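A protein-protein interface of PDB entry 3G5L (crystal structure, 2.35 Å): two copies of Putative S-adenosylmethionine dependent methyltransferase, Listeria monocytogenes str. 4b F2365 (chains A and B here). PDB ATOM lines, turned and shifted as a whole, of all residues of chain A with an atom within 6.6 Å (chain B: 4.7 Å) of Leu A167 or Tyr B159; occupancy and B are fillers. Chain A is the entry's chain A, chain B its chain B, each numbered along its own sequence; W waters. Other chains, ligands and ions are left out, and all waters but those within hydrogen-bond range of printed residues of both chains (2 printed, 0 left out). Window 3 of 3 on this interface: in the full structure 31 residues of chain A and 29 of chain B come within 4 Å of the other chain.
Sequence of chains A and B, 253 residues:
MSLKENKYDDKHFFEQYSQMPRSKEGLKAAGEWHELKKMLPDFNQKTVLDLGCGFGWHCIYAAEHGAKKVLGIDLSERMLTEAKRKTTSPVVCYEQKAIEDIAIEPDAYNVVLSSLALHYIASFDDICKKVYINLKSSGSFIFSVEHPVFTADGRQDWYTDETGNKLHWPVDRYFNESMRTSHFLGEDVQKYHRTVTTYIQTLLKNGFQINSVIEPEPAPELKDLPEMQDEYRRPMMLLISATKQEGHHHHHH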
ATOM      1  N   TRP A 158      23.562 -18.356  14.122  1.00  0.00           N
ATOM      2  CA  TRP A 158      22.766 -17.737  13.073  1.00  0.00           C
ATOM      3  C   TRP A 158      21.982 -18.765  12.277  1.00  0.00           C
ATOM      4  O   TRP A 158      22.389 -19.933  12.171  1.00  0.00           O
ATOM      5  CB  TRP A 158      23.708 -16.956  12.142  1.00  0.00           C
ATOM      6  CG  TRP A 158      24.459 -15.923  12.903  1.00  0.00           C
ATOM      7  CD1 TRP A 158      25.697 -16.051  13.468  1.00  0.00           C
ATOM      8  CD2 TRP A 158      23.986 -14.620  13.259  1.00  0.00           C
ATOM      9  NE1 TRP A 158      26.036 -14.894  14.133  1.00  0.00           N
ATOM     10  CE2 TRP A 158      25.004 -13.999  14.020  1.00  0.00           C
ATOM     11  CE3 TRP A 158      22.805 -13.909  12.997  1.00  0.00           C
ATOM     12  CZ2 TRP A 158      24.876 -12.700  14.523  1.00  0.00           C
ATOM     13  CZ3 TRP A 158      22.683 -12.613  13.492  1.00  0.00           C
ATOM     14  CH2 TRP A 158      23.713 -12.024  14.247  1.00  0.00           C
ATOM     15  N   TYR A 159      20.847 -18.336  11.736  1.00  0.00           N
ATOM     16  CA  TYR A 159      20.169 -19.136  10.738  1.00  0.00           C
ATOM     17  C   TYR A 159      20.825 -18.806   9.413  1.00  0.00           C
ATOM     18  O   TYR A 159      20.947 -17.637   9.040  1.00  0.00           O
ATOM     19  CB  TYR A 159      18.664 -18.870  10.688  1.00  0.00           C
ATOM     20  CG  TYR A 159      17.962 -19.787   9.710  1.00  0.00           C
ATOM     21  CD1 TYR A 159      17.747 -21.132  10.019  1.00  0.00           C
ATOM     22  CD2 TYR A 159      17.541 -19.322   8.463  1.00  0.00           C
ATOM     23  CE1 TYR A 159      17.115 -21.989   9.120  1.00  0.00           C
ATOM     24  CE2 TYR A 159      16.916 -20.171   7.555  1.00  0.00           C
ATOM     25  CZ  TYR A 159      16.703 -21.504   7.895  1.00  0.00           C
ATOM     26  OH  TYR A 159      16.086 -22.356   7.011  1.00  0.00           O
ATOM     27  N   THR A 160      21.275 -19.846   8.722  1.00  0.00           N
ATOM     28  CA  THR A 160      22.082 -19.684   7.520  1.00  0.00           C
ATOM     29  C   THR A 160      21.405 -20.328   6.316  1.00  0.00           C
ATOM     30  O   THR A 160      20.671 -21.315   6.462  1.00  0.00           O
ATOM     31  CB  THR A 160      23.500 -20.275   7.709  1.00  0.00           C
ATOM     32  OG1 THR A 160      23.399 -21.659   8.058  1.00  0.00           O
ATOM     33  CG2 THR A 160      24.261 -19.539   8.815  1.00  0.00           C
ATOM     34  N   ASP A 161      21.637 -19.755   5.134  1.00  0.00           N
ATOM     35  CA  ASP A 161      21.164 -20.360   3.884  1.00  0.00           C
ATOM     36  C   ASP A 161      22.188 -21.354   3.308  1.00  0.00           C
ATOM     37  O   ASP A 161      23.114 -21.771   4.009  1.00  0.00           O
ATOM     38  CB  ASP A 161      20.729 -19.292   2.854  1.00  0.00           C
ATOM     39  CG  ASP A 161      21.877 -18.393   2.375  1.00  0.00           C
ATOM     40  OD1 ASP A 161      21.591 -17.443   1.617  1.00  0.00           O
ATOM     41  OD2 ASP A 161      23.051 -18.612   2.734  1.00  0.00           O
ATOM     42  N   GLY A 164      25.555 -19.784   2.929  1.00  0.00           N
ATOM     43  CA  GLY A 164      26.103 -19.573   4.268  1.00  0.00           C
ATOM     44  C   GLY A 164      25.998 -18.165   4.831  1.00  0.00           C
ATOM     45  O   GLY A 164      26.739 -17.807   5.745  1.00  0.00           O
ATOM     46  N   ASN A 165      25.084 -17.365   4.286  1.00  0.00           N
ATOM     47  CA  ASN A 165      24.805 -16.029   4.815  1.00  0.00           C
ATOM     48  C   ASN A 165      24.006 -16.116   6.114  1.00  0.00           C
ATOM     49  O   ASN A 165      23.087 -16.925   6.219  1.00  0.00           O
ATOM     50  CB  ASN A 165      24.020 -15.194   3.798  1.00  0.00           C
ATOM     51  CG  ASN A 165      24.587 -15.294   2.393  1.00  0.00           C
ATOM     52  OD1 ASN A 165      25.795 -15.154   2.175  1.00  0.00           O
ATOM     53  ND2 ASN A 165      23.708 -15.535   1.426  1.00  0.00           N
ATOM     54  N   LYS A 166      24.365 -15.293   7.098  1.00  0.00           N
ATOM     55  CA  LYS A 166      23.592 -15.200   8.331  1.00  0.00           C
ATOM     56  C   LYS A 166      22.347 -14.400   7.992  1.00  0.00           C
ATOM     57  O   LYS A 166      22.405 -13.175   7.850  1.00  0.00           O
ATOM     58  CB  LYS A 166      24.354 -14.492   9.456  1.00  0.00           C
ATOM     59  CG  LYS A 166      25.858 -14.413   9.327  1.00  0.00           C
ATOM     60  CD  LYS A 166      26.586 -15.511  10.043  1.00  0.00           C
ATOM     61  CE  LYS A 166      28.057 -15.140  10.187  1.00  0.00           C
ATOM     62  NZ  LYS A 166      28.796 -16.055  11.093  1.00  0.00           N
ATOM     63  N   LEU A 167      21.230 -15.107   7.842  1.00  0.00           N
ATOM     64  CA  LEU A 167      19.976 -14.496   7.435  1.00  0.00           C
ATOM     65  C   LEU A 167      19.378 -13.663   8.550  1.00  0.00           C
ATOM     66  O   LEU A 167      18.955 -12.529   8.325  1.00  0.00           O
ATOM     67  CB  LEU A 167      18.975 -15.569   6.994  1.00  0.00           C
ATOM     68  CG  LEU A 167      19.297 -16.363   5.720  1.00  0.00           C
ATOM     69  CD1 LEU A 167      18.133 -17.286   5.361  1.00  0.00           C
ATOM     70  CD2 LEU A 167      19.631 -15.442   4.550  1.00  0.00           C
ATOM     71  N   HIS A 168      19.337 -14.255   9.742  1.00  0.00           N
ATOM     72  CA  HIS A 168      18.752 -13.654  10.940  1.00  0.00           C
ATOM     73  C   HIS A 168      19.113 -14.538  12.122  1.00  0.00           C
ATOM     74  O   HIS A 168      19.586 -15.662  11.934  1.00  0.00           O
ATOM     75  CB  HIS A 168      17.222 -13.557  10.828  1.00  0.00           C
ATOM     76  CG  HIS A 168      16.564 -14.840  10.421  1.00  0.00           C
ATOM     77  ND1 HIS A 168      16.085 -15.057   9.148  1.00  0.00           N
ATOM     78  CD2 HIS A 168      16.311 -15.975  11.118  1.00  0.00           C
ATOM     79  CE1 HIS A 168      15.565 -16.269   9.077  1.00  0.00           C
ATOM     80  NE2 HIS A 168      15.693 -16.848  10.257  1.00  0.00           N
ATOM     81  N   TRP A 169      18.869 -14.032  13.330  1.00  0.00           N
ATOM     82  CA  TRP A 169      19.068 -14.798  14.552  1.00  0.00           C
ATOM     83  C   TRP A 169      17.761 -15.482  14.954  1.00  0.00           C
ATOM     84  O   TRP A 169      16.768 -14.804  15.197  1.00  0.00           O
ATOM     85  CB  TRP A 169      19.552 -13.890  15.685  1.00  0.00           C
ATOM     86  CG  TRP A 169      19.932 -14.660  16.916  1.00  0.00           C
ATOM     87  CD1 TRP A 169      19.138 -14.940  17.993  1.00  0.00           C
ATOM     88  CD2 TRP A 169      21.194 -15.276  17.181  1.00  0.00           C
ATOM     89  NE1 TRP A 169      19.833 -15.678  18.913  1.00  0.00           N
ATOM     90  CE2 TRP A 169      21.098 -15.902  18.438  1.00  0.00           C
ATOM     91  CE3 TRP A 169      22.403 -15.348  16.481  1.00  0.00           C
ATOM     92  CZ2 TRP A 169      22.158 -16.599  19.007  1.00  0.00           C
ATOM     93  CZ3 TRP A 169      23.458 -16.035  17.052  1.00  0.00           C
ATOM     94  CH2 TRP A 169      23.329 -16.647  18.298  1.00  0.00           C
ATOM     95  N   ARG A 233      22.884  -6.917  15.355  1.00  0.00           N
ATOM     96  CA  ARG A 233      21.674  -7.548  14.830  1.00  0.00           C
ATOM     97  C   ARG A 233      20.868  -8.303  15.892  1.00  0.00           C
ATOM     98  O   ARG A 233      19.647  -8.416  15.791  1.00  0.00           O
ATOM     99  CB  ARG A 233      22.029  -8.442  13.635  1.00  0.00           C
ATOM    100  CG  ARG A 233      22.699  -7.662  12.481  1.00  0.00           C
ATOM    101  CD  ARG A 233      23.217  -8.597  11.397  1.00  0.00           C
ATOM    102  NE  ARG A 233      22.133  -9.321  10.743  1.00  0.00           N
ATOM    103  CZ  ARG A 233      22.283 -10.464  10.084  1.00  0.00           C
ATOM    104  NH1 ARG A 233      23.476 -11.040   9.988  1.00  0.00           N
ATOM    105  NH2 ARG A 233      21.228 -11.039   9.528  1.00  0.00           N
ATOM    106  N   ARG B 155       9.531  -7.711  10.014  1.00  0.00           N
ATOM    107  CA  ARG B 155       8.531  -8.519   9.307  1.00  0.00           C
ATOM    108  C   ARG B 155       7.373  -8.949  10.216  1.00  0.00           C
ATOM    109  O   ARG B 155       6.280  -9.271   9.732  1.00  0.00           O
ATOM    110  CB  ARG B 155       9.189  -9.717   8.597  1.00  0.00           C
ATOM    111  CG  ARG B 155       9.157 -11.054   9.335  1.00  0.00           C
ATOM    112  CD  ARG B 155      10.542 -11.667   9.386  1.00  0.00           C
ATOM    113  NE  ARG B 155      10.818 -12.646   8.339  1.00  0.00           N
ATOM    114  CZ  ARG B 155      12.041 -12.941   7.894  1.00  0.00           C
ATOM    115  NH1 ARG B 155      13.109 -12.317   8.380  1.00  0.00           N
ATOM    116  NH2 ARG B 155      12.200 -13.853   6.947  1.00  0.00           N
ATOM    117  N   ASP B 157       6.569 -11.566  11.984  1.00  0.00           N
ATOM    118  CA  ASP B 157       5.982 -12.838  11.581  1.00  0.00           C
ATOM    119  C   ASP B 157       7.085 -13.872  11.763  1.00  0.00           C
ATOM    120  O   ASP B 157       8.264 -13.521  11.859  1.00  0.00           O
ATOM    121  CB  ASP B 157       5.544 -12.769  10.101  1.00  0.00           C
ATOM    122  CG  ASP B 157       4.527 -13.857   9.702  1.00  0.00           C
ATOM    123  OD1 ASP B 157       3.956 -14.545  10.573  1.00  0.00           O
ATOM    124  OD2 ASP B 157       4.294 -14.012   8.486  1.00  0.00           O
ATOM    125  N   TRP B 158       6.692 -15.140  11.794  1.00  0.00           N
ATOM    126  CA  TRP B 158       7.606 -16.278  11.859  1.00  0.00           C
ATOM    127  C   TRP B 158       8.474 -16.430  10.615  1.00  0.00           C
ATOM    128  O   TRP B 158       8.218 -15.803   9.580  1.00  0.00           O
ATOM    129  CB  TRP B 158       6.801 -17.565  12.064  1.00  0.00           C
ATOM    130  CG  TRP B 158       5.968 -17.512  13.304  1.00  0.00           C
ATOM    131  CD1 TRP B 158       4.680 -17.076  13.410  1.00  0.00           C
ATOM    132  CD2 TRP B 158       6.378 -17.884  14.625  1.00  0.00           C
ATOM    133  NE1 TRP B 158       4.256 -17.168  14.715  1.00  0.00           N
ATOM    134  CE2 TRP B 158       5.279 -17.658  15.482  1.00  0.00           C
ATOM    135  CE3 TRP B 158       7.564 -18.401  15.166  1.00  0.00           C
ATOM    136  CZ2 TRP B 158       5.334 -17.917  16.854  1.00  0.00           C
ATOM    137  CZ3 TRP B 158       7.616 -18.665  16.526  1.00  0.00           C
ATOM    138  CH2 TRP B 158       6.509 -18.418  17.355  1.00  0.00           C
ATOM    139  N   TYR B 159       9.517 -17.249  10.732  1.00  0.00           N
ATOM    140  CA  TYR B 159      10.231 -17.728   9.561  1.00  0.00           C
ATOM    141  C   TYR B 159       9.638 -19.067   9.149  1.00  0.00           C
ATOM    142  O   TYR B 159       9.430 -19.948   9.984  1.00  0.00           O
ATOM    143  CB  TYR B 159      11.727 -17.869   9.813  1.00  0.00           C
ATOM    144  CG  TYR B 159      12.494 -18.158   8.545  1.00  0.00           C
ATOM    145  CD1 TYR B 159      12.710 -17.157   7.599  1.00  0.00           C
ATOM    146  CD2 TYR B 159      12.982 -19.434   8.276  1.00  0.00           C
ATOM    147  CE1 TYR B 159      13.409 -17.408   6.429  1.00  0.00           C
ATOM    148  CE2 TYR B 159      13.670 -19.701   7.096  1.00  0.00           C
ATOM    149  CZ  TYR B 159      13.887 -18.679   6.181  1.00  0.00           C
ATOM    150  OH  TYR B 159      14.577 -18.921   5.014  1.00  0.00           O
ATOM    151  N   THR B 160       9.307 -19.202   7.893  1.00  0.00           N
ATOM    152  CA  THR B 160       8.626 -20.388   7.447  1.00  0.00           C
ATOM    153  C   THR B 160       9.427 -21.003   6.371  1.00  0.00           C
ATOM    154  O   THR B 160      10.147 -20.336   5.686  1.00  0.00           O
ATOM    155  CB  THR B 160       7.219 -20.092   6.967  1.00  0.00           C
ATOM    156  OG1 THR B 160       7.275 -19.100   5.960  1.00  0.00           O
ATOM    157  CG2 THR B 160       6.378 -19.581   8.102  1.00  0.00           C
ATOM    158  N   ASP B 161       9.324 -22.300   6.224  1.00  0.00           N
ATOM    159  CA  ASP B 161       9.850 -22.906   5.024  1.00  0.00           C
ATOM    160  C   ASP B 161       8.825 -22.966   3.941  1.00  0.00           C
ATOM    161  O   ASP B 161       7.745 -22.448   4.085  1.00  0.00           O
ATOM    162  CB  ASP B 161      10.416 -24.284   5.291  1.00  0.00           C
ATOM    163  CG  ASP B 161       9.405 -25.232   5.797  1.00  0.00           C
ATOM    164  OD1 ASP B 161       8.944 -25.058   6.907  1.00  0.00           O
ATOM    165  OD2 ASP B 161       9.092 -26.189   5.096  1.00  0.00           O
ATOM    166  N   ASN B 165       5.303 -24.514   7.687  1.00  0.00           N
ATOM    167  CA  ASN B 165       5.748 -24.691   9.046  1.00  0.00           C
ATOM    168  C   ASN B 165       6.399 -23.465   9.656  1.00  0.00           C
ATOM    169  O   ASN B 165       7.205 -22.840   9.040  1.00  0.00           O
ATOM    170  CB  ASN B 165       6.636 -25.916   9.141  1.00  0.00           C
ATOM    171  CG  ASN B 165       5.918 -27.152   8.744  1.00  0.00           C
ATOM    172  OD1 ASN B 165       4.815 -27.382   9.193  1.00  0.00           O
ATOM    173  ND2 ASN B 165       6.524 -27.956   7.864  1.00  0.00           N
ATOM    174  N   LYS B 166       6.002 -23.128  10.868  1.00  0.00           N
ATOM    175  CA  LYS B 166       6.640 -22.025  11.586  1.00  0.00           C
ATOM    176  C   LYS B 166       7.895 -22.563  12.267  1.00  0.00           C
ATOM    177  O   LYS B 166       7.815 -23.310  13.248  1.00  0.00           O
ATOM    178  CB  LYS B 166       5.666 -21.405  12.589  1.00  0.00           C
ATOM    179  CG  LYS B 166       4.425 -20.819  11.932  1.00  0.00           C
ATOM    180  CD  LYS B 166       3.366 -20.461  12.952  1.00  0.00           C
ATOM    181  CE  LYS B 166       2.087 -20.003  12.265  1.00  0.00           C
ATOM    182  NZ  LYS B 166       1.147 -19.365  13.232  1.00  0.00           N
ATOM    183  N   LEU B 167       9.047 -22.207  11.704  1.00  0.00           N
ATOM    184  CA  LEU B 167      10.330 -22.809  12.062  1.00  0.00           C
ATOM    185  C   LEU B 167      10.864 -22.264  13.382  1.00  0.00           C
ATOM    186  O   LEU B 167      11.245 -23.030  14.271  1.00  0.00           O
ATOM    187  CB  LEU B 167      11.349 -22.575  10.935  1.00  0.00           C
ATOM    188  CG  LEU B 167      11.747 -23.662   9.920  1.00  0.00           C
ATOM    189  CD1 LEU B 167      10.682 -24.739   9.667  1.00  0.00           C
ATOM    190  CD2 LEU B 167      12.171 -23.003   8.609  1.00  0.00           C
ATOM    191  N   HIS B 168      10.874 -20.937  13.485  1.00  0.00           N
ATOM    192  CA  HIS B 168      11.363 -20.189  14.641  1.00  0.00           C
ATOM    193  C   HIS B 168      11.010 -18.741  14.381  1.00  0.00           C
ATOM    194  O   HIS B 168      10.555 -18.401  13.288  1.00  0.00           O
ATOM    195  CB  HIS B 168      12.890 -20.315  14.792  1.00  0.00           C
ATOM    196  CG  HIS B 168      13.651 -20.054  13.528  1.00  0.00           C
ATOM    197  ND1 HIS B 168      14.121 -21.069  12.724  1.00  0.00           N
ATOM    198  CD2 HIS B 168      14.012 -18.897  12.923  1.00  0.00           C
ATOM    199  CE1 HIS B 168      14.748 -20.549  11.684  1.00  0.00           C
ATOM    200  NE2 HIS B 168      14.696 -19.233  11.780  1.00  0.00           N
ATOM    201  N   PRO B 170      12.316 -14.967  13.801  1.00  0.00           N
ATOM    202  CA  PRO B 170      13.531 -14.277  13.385  1.00  0.00           C
ATOM    203  C   PRO B 170      13.782 -12.965  14.120  1.00  0.00           C
ATOM    204  O   PRO B 170      12.868 -12.143  14.294  1.00  0.00           O
ATOM    205  CB  PRO B 170      13.308 -14.037  11.891  1.00  0.00           C
ATOM    206  CG  PRO B 170      11.836 -14.045  11.708  1.00  0.00           C
ATOM    207  CD  PRO B 170      11.189 -14.706  12.890  1.00  0.00           C
ATOM    208  N   ASP B 172      16.491  -9.688  13.964  1.00  0.00           N
ATOM    209  CA  ASP B 172      17.507  -8.980  13.205  1.00  0.00           C
ATOM    210  C   ASP B 172      17.414  -7.500  13.554  1.00  0.00           C
ATOM    211  O   ASP B 172      16.415  -7.073  14.116  1.00  0.00           O
ATOM    212  CB  ASP B 172      17.306  -9.190  11.699  1.00  0.00           C
ATOM    213  CG  ASP B 172      18.601  -9.077  10.906  1.00  0.00           C
ATOM    214  OD1 ASP B 172      19.514  -8.331  11.327  1.00  0.00           O
ATOM    215  OD2 ASP B 172      18.703  -9.745   9.853  1.00  0.00           O
HETATM  216  O   HOH W   1      15.954 -13.117   7.449  1.00  0.00           O
HETATM  217  O   HOH W   2      16.266 -10.433   8.651  1.00  0.00           O
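Of the printed residues of chain B, Tyr A159 touches Tyr B159 and His B168. Leu A167 touches two residues of chain B. Printed residues of chain B within 4 Å of His A168: Tyr B159, His B168 and Pro B170. Of the printed residues of chain B, Trp A169 touches Pro B170. Of the printed residues of chain A, His B168 touches Tyr A159 (3.5 Å) and His A168 (3.0 Å). Of the printed residues of chain A, Pro B170 touches His A168 and Trp A169. The nearest printed residue of chain B that does not touch Leu A167 is Arg B155 (5.9 Å).
The backbone carbonyl oxygen (O) of Tyr A159 sits at hydrogen-bond distance from the backbone NH (N) of Leu A167, 2.8 Å away. The backbone carbonyl oxygen (O) of His A168 sits at hydrogen-bond distance from the backbone NH (N) of Tyr A159, at 3.0 Å. The backbone carbonyl oxygen (O) of Lys A166 lies within hydrogen-bond range of the guanidinium group (NH2) of Arg A233 (3.0 Å). The guanidinium group (NH2) of Arg A233 sits at hydrogen-bond distance from the backbone carbonyl oxygen (O) of Leu A167 (3.0 Å). O of Tyr B159 is in hydrogen-bond range of N of Leu B167. The backbone NH of Tyr B159 lies within hydrogen-bond range of the backbone carbonyl oxygen of His B168 (3.0 Å).
Tyr B159 touches its own counterpart, Tyr A159. Tyr A159 touches His B168, and with the chains exchanged His A168 touches Tyr B159. Leu A167 touches Tyr B159, but with the chains exchanged Tyr A159 does not touch Leu B167 (4.3 Å). His A168 touches its own counterpart, His B168. 8 positions are printed for both chains.
Printed residues of chain B that touch a printed residue of chain A: Tyr B159, His B168, Pro B170 and Asp B172. Printed residues of chain A that touch a printed residue of chain B: Tyr A159, Leu A167, His A168, Trp A169 and Arg A233. Hydrophobic or aromatic side chains of chain A within 4 Å of the printed part of chain B: Tyr A159, Leu A167 and His A168. Among the printed residues, 9 pairs touch across the chains.
A ring nitrogen (NE2) of His A168 sits at hydrogen-bond distance from a ring nitrogen (NE2) of His B168, 3.0 Å away. OD2 of Asp B172 is in salt-bridge range of NH2 of Arg A233. O of Leu A167 lies close to OD2 of Asp B172 (3.2 Å).
CE2 of Tyr B159 touches CE2 of Tyr A159, at 3.3 Å. His B168 touches Tyr A159. Tyr B159 touches Leu A167. CD1 of Tyr B159 touches CE1 of His A168, at 3.3 Å. His A168 touches Pro B170. Pro B170 touches Trp A169 (C to O, 3.7 Å).
Water W1 lies within hydrogen-bond range of ND1 of His A168 (2.6 Å), NH1 of Arg B155 (3.1 Å) and O of Leu A167 (3.2 Å). Water W2 lies within hydrogen-bond range of the side-chain carboxylate of Asp B172 (2.8 Å) and the backbone carbonyl oxygen of Leu A167 (3.4 Å).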
